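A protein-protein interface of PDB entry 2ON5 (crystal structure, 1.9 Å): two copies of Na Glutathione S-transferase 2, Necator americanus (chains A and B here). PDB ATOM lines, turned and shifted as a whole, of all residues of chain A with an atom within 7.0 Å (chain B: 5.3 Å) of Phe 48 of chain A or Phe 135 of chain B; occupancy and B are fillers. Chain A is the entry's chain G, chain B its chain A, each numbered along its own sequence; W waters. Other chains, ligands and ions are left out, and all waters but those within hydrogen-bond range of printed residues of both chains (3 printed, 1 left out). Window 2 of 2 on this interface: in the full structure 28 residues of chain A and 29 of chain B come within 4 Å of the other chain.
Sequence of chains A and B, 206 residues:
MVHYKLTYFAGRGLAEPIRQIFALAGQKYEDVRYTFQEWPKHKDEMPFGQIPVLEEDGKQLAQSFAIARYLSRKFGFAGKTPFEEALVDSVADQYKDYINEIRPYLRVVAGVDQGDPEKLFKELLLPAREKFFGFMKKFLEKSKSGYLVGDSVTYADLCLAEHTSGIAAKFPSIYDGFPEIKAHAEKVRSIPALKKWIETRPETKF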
ATOM      1  N   TRP A  39      12.384  -4.195  14.060  1.00  0.00           N
ATOM      2  CA  TRP A  39      11.987  -5.597  13.912  1.00  0.00           C
ATOM      3  C   TRP A  39      10.607  -5.972  14.494  1.00  0.00           C
ATOM      4  O   TRP A  39       9.829  -6.631  13.812  1.00  0.00           O
ATOM      5  CB  TRP A  39      13.095  -6.491  14.489  1.00  0.00           C
ATOM      6  CG  TRP A  39      12.693  -7.892  14.877  1.00  0.00           C
ATOM      7  CD1 TRP A  39      12.769  -8.437  16.122  1.00  0.00           C
ATOM      8  CD2 TRP A  39      12.169  -8.921  14.017  1.00  0.00           C
ATOM      9  NE1 TRP A  39      12.337  -9.742  16.098  1.00  0.00           N
ATOM     10  CE2 TRP A  39      11.958 -10.065  14.820  1.00  0.00           C
ATOM     11  CE3 TRP A  39      11.853  -8.986  12.654  1.00  0.00           C
ATOM     12  CZ2 TRP A  39      11.443 -11.262  14.306  1.00  0.00           C
ATOM     13  CZ3 TRP A  39      11.336 -10.190  12.141  1.00  0.00           C
ATOM     14  CH2 TRP A  39      11.134 -11.301  12.966  1.00  0.00           C
ATOM     15  N   LYS A  43       7.562  -9.101  13.113  1.00  0.00           N
ATOM     16  CA  LYS A  43       7.723 -10.429  13.697  1.00  0.00           C
ATOM     17  C   LYS A  43       6.650 -11.416  13.210  1.00  0.00           C
ATOM     18  O   LYS A  43       6.967 -12.520  12.740  1.00  0.00           O
ATOM     19  CB  LYS A  43       7.711 -10.295  15.223  1.00  0.00           C
ATOM     20  CG  LYS A  43       8.061 -11.526  15.978  1.00  0.00           C
ATOM     21  CD  LYS A  43       7.773 -11.307  17.456  1.00  0.00           C
ATOM     22  CE  LYS A  43       8.707 -12.075  18.349  1.00  0.00           C
ATOM     23  NZ  LYS A  43       8.989 -13.449  17.893  1.00  0.00           N
ATOM     24  N   GLU A  45       4.843 -11.478  10.567  1.00  0.00           N
ATOM     25  CA  GLU A  45       4.950 -11.851   9.137  1.00  0.00           C
ATOM     26  C   GLU A  45       5.716 -13.163   8.927  1.00  0.00           C
ATOM     27  O   GLU A  45       5.624 -13.779   7.869  1.00  0.00           O
ATOM     28  CB  GLU A  45       5.684 -10.768   8.347  1.00  0.00           C
ATOM     29  CG  GLU A  45       5.113  -9.379   8.520  1.00  0.00           C
ATOM     30  CD  GLU A  45       5.962  -8.322   7.854  1.00  0.00           C
ATOM     31  OE1 GLU A  45       6.702  -8.644   6.891  1.00  0.00           O
ATOM     32  OE2 GLU A  45       5.883  -7.155   8.288  1.00  0.00           O
ATOM     33  N   MET A  46       6.483 -13.578   9.929  1.00  0.00           N
ATOM     34  CA  MET A  46       7.484 -14.641   9.721  1.00  0.00           C
ATOM     35  C   MET A  46       6.962 -16.021  10.154  1.00  0.00           C
ATOM     36  O   MET A  46       6.193 -16.117  11.122  1.00  0.00           O
ATOM     37  CB  MET A  46       8.814 -14.287  10.415  1.00  0.00           C
ATOM     38  CG  MET A  46       9.379 -12.902  10.060  1.00  0.00           C
ATOM     39  SD  MET A  46       9.452 -12.661   8.277  1.00  0.00           S
ATOM     40  CE  MET A  46       9.891 -10.930   8.165  1.00  0.00           C
ATOM     41  N   PRO A  47       7.345 -17.097   9.424  1.00  0.00           N
ATOM     42  CA  PRO A  47       6.802 -18.431   9.750  1.00  0.00           C
ATOM     43  C   PRO A  47       6.943 -18.825  11.221  1.00  0.00           C
ATOM     44  O   PRO A  47       6.016 -19.400  11.814  1.00  0.00           O
ATOM     45  CB  PRO A  47       7.625 -19.372   8.864  1.00  0.00           C
ATOM     46  CG  PRO A  47       7.937 -18.536   7.662  1.00  0.00           C
ATOM     47  CD  PRO A  47       8.221 -17.142   8.237  1.00  0.00           C
ATOM     48  N   PHE A  48       8.097 -18.557  11.799  1.00  0.00           N
ATOM     49  CA  PHE A  48       8.291 -18.845  13.206  1.00  0.00           C
ATOM     50  C   PHE A  48       8.512 -17.576  14.018  1.00  0.00           C
ATOM     51  O   PHE A  48       9.047 -17.630  15.123  1.00  0.00           O
ATOM     52  CB  PHE A  48       9.439 -19.832  13.390  1.00  0.00           C
ATOM     53  CG  PHE A  48       9.317 -21.070  12.523  1.00  0.00           C
ATOM     54  CD1 PHE A  48      10.244 -21.324  11.506  1.00  0.00           C
ATOM     55  CD2 PHE A  48       8.260 -21.974  12.706  1.00  0.00           C
ATOM     56  CE1 PHE A  48      10.113 -22.491  10.695  1.00  0.00           C
ATOM     57  CE2 PHE A  48       8.137 -23.160  11.887  1.00  0.00           C
ATOM     58  CZ  PHE A  48       9.082 -23.396  10.889  1.00  0.00           C
ATOM     59  N   GLY A  49       8.101 -16.440  13.468  1.00  0.00           N
ATOM     60  CA  GLY A  49       8.296 -15.161  14.160  1.00  0.00           C
ATOM     61  C   GLY A  49       9.759 -14.862  14.459  1.00  0.00           C
ATOM     62  O   GLY A  49      10.082 -14.163  15.413  1.00  0.00           O
ATOM     63  N   GLN A  50      10.646 -15.373  13.612  1.00  0.00           N
ATOM     64  CA  GLN A  50      12.085 -15.132  13.737  1.00  0.00           C
ATOM     65  C   GLN A  50      12.682 -14.824  12.358  1.00  0.00           C
ATOM     66  O   GLN A  50      12.024 -15.003  11.344  1.00  0.00           O
ATOM     67  CB  GLN A  50      12.793 -16.317  14.435  1.00  0.00           C
ATOM     68  CG  GLN A  50      12.549 -16.258  15.959  1.00  0.00           C
ATOM     69  CD  GLN A  50      13.549 -17.041  16.789  1.00  0.00           C
ATOM     70  OE1 GLN A  50      13.664 -18.264  16.662  1.00  0.00           O
ATOM     71  NE2 GLN A  50      14.257 -16.338  17.676  1.00  0.00           N
ATOM     72  N   ILE A  51      13.908 -14.312  12.355  1.00  0.00           N
ATOM     73  CA  ILE A  51      14.673 -14.080  11.124  1.00  0.00           C
ATOM     74  C   ILE A  51      16.026 -14.772  11.283  1.00  0.00           C
ATOM     75  O   ILE A  51      16.455 -14.997  12.412  1.00  0.00           O
ATOM     76  CB  ILE A  51      14.840 -12.563  10.825  1.00  0.00           C
ATOM     77  CG1 ILE A  51      15.073 -11.753  12.111  1.00  0.00           C
ATOM     78  CG2 ILE A  51      13.639 -12.066  10.018  1.00  0.00           C
ATOM     79  CD1 ILE A  51      15.202 -10.223  11.872  1.00  0.00           C
ATOM     80  N   VAL A  53      14.693 -14.930   7.095  1.00  0.00           N
ATOM     81  CA  VAL A  53      13.671 -15.566   6.257  1.00  0.00           C
ATOM     82  C   VAL A  53      13.939 -15.183   4.812  1.00  0.00           C
ATOM     83  O   VAL A  53      14.189 -14.003   4.486  1.00  0.00           O
ATOM     84  CB  VAL A  53      12.250 -15.090   6.636  1.00  0.00           C
ATOM     85  CG1 VAL A  53      11.211 -15.536   5.592  1.00  0.00           C
ATOM     86  CG2 VAL A  53      11.885 -15.592   8.023  1.00  0.00           C
ATOM     87  N   LEU A  61      10.639 -19.007   3.277  1.00  0.00           N
ATOM     88  CA  LEU A  61      11.378 -20.111   3.861  1.00  0.00           C
ATOM     89  C   LEU A  61      12.214 -19.536   4.993  1.00  0.00           C
ATOM     90  O   LEU A  61      13.088 -18.662   4.770  1.00  0.00           O
ATOM     91  CB  LEU A  61      12.304 -20.746   2.823  1.00  0.00           C
ATOM     92  CG  LEU A  61      13.297 -21.775   3.361  1.00  0.00           C
ATOM     93  CD1 LEU A  61      12.564 -22.998   3.878  1.00  0.00           C
ATOM     94  CD2 LEU A  61      14.313 -22.146   2.243  1.00  0.00           C
ATOM     95  N   ALA A  62      11.937 -20.022   6.194  1.00  0.00           N
ATOM     96  CA  ALA A  62      12.682 -19.631   7.387  1.00  0.00           C
ATOM     97  C   ALA A  62      13.746 -20.650   7.731  1.00  0.00           C
ATOM     98  O   ALA A  62      13.878 -21.693   7.067  1.00  0.00           O
ATOM     99  CB  ALA A  62      11.740 -19.491   8.563  1.00  0.00           C
ATOM    100  N   GLN A  63      14.482 -20.322   8.789  1.00  0.00           N
ATOM    101  CA  GLN A  63      15.473 -21.163   9.449  1.00  0.00           C
ATOM    102  C   GLN A  63      16.778 -21.127   8.635  1.00  0.00           C
ATOM    103  O   GLN A  63      16.841 -21.635   7.516  1.00  0.00           O
ATOM    104  CB  GLN A  63      14.931 -22.592   9.708  1.00  0.00           C
ATOM    105  CG  GLN A  63      13.985 -22.679  10.913  1.00  0.00           C
ATOM    106  CD  GLN A  63      14.714 -22.588  12.258  1.00  0.00           C
ATOM    107  OE1 GLN A  63      14.080 -22.509  13.336  1.00  0.00           O
ATOM    108  NE2 GLN A  63      16.035 -22.650  12.212  1.00  0.00           N
ATOM    109  N   SER B  90      13.046 -26.664   7.414  1.00  0.00           N
ATOM    110  CA  SER B  90      12.738 -25.514   8.312  1.00  0.00           C
ATOM    111  C   SER B  90      11.883 -25.931   9.525  1.00  0.00           C
ATOM    112  O   SER B  90      12.126 -25.462  10.651  1.00  0.00           O
ATOM    113  CB  SER B  90      12.068 -24.370   7.519  1.00  0.00           C
ATOM    114  OG  SER B  90      10.716 -24.648   7.212  1.00  0.00           O
ATOM    115  N   VAL B  91      10.905 -26.816   9.297  1.00  0.00           N
ATOM    116  CA  VAL B  91      10.099 -27.394  10.383  1.00  0.00           C
ATOM    117  C   VAL B  91      10.961 -28.229  11.325  1.00  0.00           C
ATOM    118  O   VAL B  91      10.826 -28.114  12.576  1.00  0.00           O
ATOM    119  CB  VAL B  91       8.867 -28.230   9.855  1.00  0.00           C
ATOM    120  CG1 VAL B  91       8.116 -28.925  11.023  1.00  0.00           C
ATOM    121  CG2 VAL B  91       7.881 -27.317   9.104  1.00  0.00           C
ATOM    122  N   GLN B  94      12.963 -25.929  13.416  1.00  0.00           N
ATOM    123  CA  GLN B  94      12.151 -25.342  14.498  1.00  0.00           C
ATOM    124  C   GLN B  94      11.925 -26.353  15.650  1.00  0.00           C
ATOM    125  O   GLN B  94      12.018 -26.004  16.853  1.00  0.00           O
ATOM    126  CB  GLN B  94      10.809 -24.809  13.972  1.00  0.00           C
ATOM    127  CG  GLN B  94       9.986 -24.077  15.061  1.00  0.00           C
ATOM    128  CD  GLN B  94      10.550 -22.683  15.348  1.00  0.00           C
ATOM    129  OE1 GLN B  94      11.444 -22.202  14.648  1.00  0.00           O
ATOM    130  NE2 GLN B  94      10.036 -22.033  16.403  1.00  0.00           N
ATOM    131  N   LYS B 131       4.231 -22.243  22.400  1.00  0.00           N
ATOM    132  CA  LYS B 131       4.821 -21.507  21.265  1.00  0.00           C
ATOM    133  C   LYS B 131       5.015 -22.462  20.102  1.00  0.00           C
ATOM    134  O   LYS B 131       4.588 -22.177  18.989  1.00  0.00           O
ATOM    135  CB  LYS B 131       6.184 -20.907  21.623  1.00  0.00           C
ATOM    136  CG  LYS B 131       6.153 -19.710  22.607  1.00  0.00           C
ATOM    137  CD  LYS B 131       7.574 -19.266  23.028  1.00  0.00           C
ATOM    138  CE  LYS B 131       8.258 -20.316  23.909  1.00  0.00           C
ATOM    139  NZ  LYS B 131       9.698 -19.986  24.178  1.00  0.00           N
ATOM    140  N   PHE B 132       5.663 -23.599  20.377  1.00  0.00           N
ATOM    141  CA  PHE B 132       6.051 -24.523  19.306  1.00  0.00           C
ATOM    142  C   PHE B 132       4.849 -25.112  18.564  1.00  0.00           C
ATOM    143  O   PHE B 132       4.779 -25.024  17.325  1.00  0.00           O
ATOM    144  CB  PHE B 132       6.992 -25.602  19.832  1.00  0.00           C
ATOM    145  CG  PHE B 132       7.365 -26.638  18.797  1.00  0.00           C
ATOM    146  CD1 PHE B 132       7.169 -27.977  19.060  1.00  0.00           C
ATOM    147  CD2 PHE B 132       7.895 -26.261  17.563  1.00  0.00           C
ATOM    148  CE1 PHE B 132       7.479 -28.936  18.104  1.00  0.00           C
ATOM    149  CE2 PHE B 132       8.245 -27.213  16.610  1.00  0.00           C
ATOM    150  CZ  PHE B 132       8.026 -28.559  16.880  1.00  0.00           C
ATOM    151  N   PHE B 133       3.901 -25.674  19.329  1.00  0.00           N
ATOM    152  CA  PHE B 133       2.689 -26.289  18.768  1.00  0.00           C
ATOM    153  C   PHE B 133       1.858 -25.241  18.023  1.00  0.00           C
ATOM    154  O   PHE B 133       1.078 -25.567  17.125  1.00  0.00           O
ATOM    155  CB  PHE B 133       1.837 -26.931  19.867  1.00  0.00           C
ATOM    156  CG  PHE B 133       2.404 -28.223  20.450  1.00  0.00           C
ATOM    157  CD1 PHE B 133       3.688 -28.671  20.140  1.00  0.00           C
ATOM    158  CD2 PHE B 133       1.622 -28.983  21.320  1.00  0.00           C
ATOM    159  CE1 PHE B 133       4.159 -29.843  20.710  1.00  0.00           C
ATOM    160  CE2 PHE B 133       2.103 -30.139  21.929  1.00  0.00           C
ATOM    161  CZ  PHE B 133       3.360 -30.576  21.608  1.00  0.00           C
ATOM    162  N   GLY B 134       2.002 -23.979  18.416  1.00  0.00           N
ATOM    163  CA  GLY B 134       1.320 -22.874  17.721  1.00  0.00           C
ATOM    164  C   GLY B 134       1.825 -22.732  16.289  1.00  0.00           C
ATOM    165  O   GLY B 134       1.037 -22.540  15.366  1.00  0.00           O
ATOM    166  N   PHE B 135       3.139 -22.829  16.093  1.00  0.00           N
ATOM    167  CA  PHE B 135       3.698 -22.805  14.739  1.00  0.00           C
ATOM    168  C   PHE B 135       3.353 -24.055  13.929  1.00  0.00           C
ATOM    169  O   PHE B 135       3.099 -23.962  12.735  1.00  0.00           O
ATOM    170  CB  PHE B 135       5.204 -22.545  14.754  1.00  0.00           C
ATOM    171  CG  PHE B 135       5.582 -21.212  15.362  1.00  0.00           C
ATOM    172  CD1 PHE B 135       6.439 -21.144  16.448  1.00  0.00           C
ATOM    173  CD2 PHE B 135       5.043 -20.036  14.867  1.00  0.00           C
ATOM    174  CE1 PHE B 135       6.790 -19.896  17.023  1.00  0.00           C
ATOM    175  CE2 PHE B 135       5.379 -18.788  15.441  1.00  0.00           C
ATOM    176  CZ  PHE B 135       6.253 -18.728  16.517  1.00  0.00           C
ATOM    177  N   MET B 136       3.350 -25.212  14.580  1.00  0.00           N
ATOM    178  CA  MET B 136       3.009 -26.488  13.928  1.00  0.00           C
ATOM    179  C   MET B 136       1.556 -26.498  13.435  1.00  0.00           C
ATOM    180  O   MET B 136       1.264 -26.997  12.348  1.00  0.00           O
ATOM    181  CB  MET B 136       3.282 -27.667  14.868  1.00  0.00           C
ATOM    182  CG  MET B 136       4.766 -27.876  15.214  1.00  0.00           C
ATOM    183  SD  MET B 136       5.905 -27.918  13.798  1.00  0.00           S
ATOM    184  CE  MET B 136       6.429 -26.213  13.636  1.00  0.00           C
ATOM    185  N   LYS B 137       0.670 -25.941  14.255  1.00  0.00           N
ATOM    186  CA  LYS B 137      -0.727 -25.703  13.905  1.00  0.00           C
ATOM    187  C   LYS B 137      -0.833 -24.885  12.606  1.00  0.00           C
ATOM    188  O   LYS B 137      -1.596 -25.232  11.715  1.00  0.00           O
ATOM    189  CB  LYS B 137      -1.424 -25.011  15.095  1.00  0.00           C
ATOM    190  CG  LYS B 137      -2.931 -24.885  15.041  1.00  0.00           C
ATOM    191  CD  LYS B 137      -3.408 -24.133  16.316  1.00  0.00           C
ATOM    192  CE  LYS B 137      -4.905 -24.015  16.367  1.00  0.00           C
ATOM    193  NZ  LYS B 137      -5.277 -23.562  17.740  1.00  0.00           N
ATOM    194  N   LYS B 138      -0.022 -23.839  12.482  1.00  0.00           N
ATOM    195  CA  LYS B 138       0.014 -23.032  11.268  1.00  0.00           C
ATOM    196  C   LYS B 138       0.397 -23.822  10.033  1.00  0.00           C
ATOM    197  O   LYS B 138      -0.179 -23.627   8.963  1.00  0.00           O
ATOM    198  CB  LYS B 138       0.992 -21.873  11.416  1.00  0.00           C
ATOM    199  CG  LYS B 138       0.572 -20.845  12.439  1.00  0.00           C
ATOM    200  CD  LYS B 138       1.718 -19.820  12.705  1.00  0.00           C
ATOM    201  CE  LYS B 138       2.550 -19.492  11.437  1.00  0.00           C
ATOM    202  NZ  LYS B 138       3.342 -18.236  11.583  1.00  0.00           N
ATOM    203  N   PHE B 139       1.404 -24.684  10.173  1.00  0.00           N
ATOM    204  CA  PHE B 139       1.857 -25.510   9.051  1.00  0.00           C
ATOM    205  C   PHE B 139       0.797 -26.515   8.635  1.00  0.00           C
ATOM    206  O   PHE B 139       0.563 -26.709   7.425  1.00  0.00           O
ATOM    207  CB  PHE B 139       3.211 -26.155   9.349  1.00  0.00           C
ATOM    208  CG  PHE B 139       4.350 -25.269   8.999  1.00  0.00           C
ATOM    209  CD1 PHE B 139       4.690 -24.195   9.825  1.00  0.00           C
ATOM    210  CD2 PHE B 139       5.040 -25.441   7.810  1.00  0.00           C
ATOM    211  CE1 PHE B 139       5.708 -23.324   9.482  1.00  0.00           C
ATOM    212  CE2 PHE B 139       6.085 -24.554   7.448  1.00  0.00           C
ATOM    213  CZ  PHE B 139       6.415 -23.505   8.287  1.00  0.00           C
HETATM  214  O   HOH W   1       3.153 -15.401   9.720  1.00  0.00           O
HETATM  215  O   HOH W   2       9.743 -22.009   6.673  1.00  0.00           O
HETATM  216  O   HOH W   3      10.787 -19.177  16.912  1.00  0.00           O
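The side-chain amide oxygen (OE1) of Gln 63 of chain A sits close to the side-chain amide oxygen (OE1) of Gln 94 of chain B (3.0 Å).
The side-chain amino group (NZ) of Lys 138 of chain B is in hydrogen-bond range of the backbone carbonyl oxygen (O) of Pro 47 of chain A, 2.9 Å away.
No position is printed for both chains.
Of the 12 pairs that touch across the chains among the printed residues, none has its exchanged pair printed and touching as well.
Among the printed residues, pairs that only touch across the chains: Met 46 of chain A with Lys 138 of chain B (3.6 Å), Pro 47 of chain A with Phe 135 of chain B (3.3 Å), Phe 48 of chain A with Ser 90 of chain B (3.6 Å), Phe 48 of chain A with Gln 94 of chain B (3.2 Å), Phe 48 of chain A with Phe 135 of chain B (3.3 Å), Phe 48 of chain A with Met 136 of chain B (3.9 Å), Phe 48 of chain A with Phe 139 of chain B (3.4 Å), Leu 61 of chain A with Ser 90 of chain B (3.9 Å), Ala 62 of chain A with Ser 90 of chain B (3.3 Å) and Gln 63 of chain A with Ser 90 of chain B (3.4 Å).
Hydrophobic or aromatic side chains of chain A within 4 Å of the printed part of chain B: Phe 48 and Leu 61.
Water W2 bridges the side-chain hydroxyl of Ser 90 of chain B and the backbone NH of Ala 62 of chain A.
Water W3 lies within hydrogen-bond range of O of Phe 48 of chain A (2.9 Å), NE2 of Gln 94 of chain B (3.0 Å) and OE1 of Gln 50 of chain A (3.0 Å).
Water W1 lies within hydrogen-bond range of NZ of Lys 138 of chain B (3.4 Å), O of Met 46 of chain A (3.4 Å) and O of Glu 45 of chain A (3.5 Å).
Of chain B, only Ser 90, Gln 94, Phe 135, Met 136 and Phe 139 come within 4 Å of Phe 48 of chain A.
Phe 135 of chain B touches just these residues of chain A: Pro 47 and Phe 48.
Of the printed residues of chain A, Met 136 of chain B touches Phe 48 (3.9 Å).
Of the printed residues of chain A, Phe 139 of chain B touches Phe 48.
Of the printed residues of chain A, Lys 138 of chain B touches Met 46 and Pro 47.
Phe 133 of chain B touches none of the printed residues of chain A.
Val 53 of chain A touches none of the printed residues of chain B.
The nearest residue of chain B that does not touch Phe 48 of chain A is Val 91 of chain B (4.2 Å).
The nearest printed residue of chain A that does not touch Met 136 of chain B is Pro 47 of chain A (7.0 Å).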
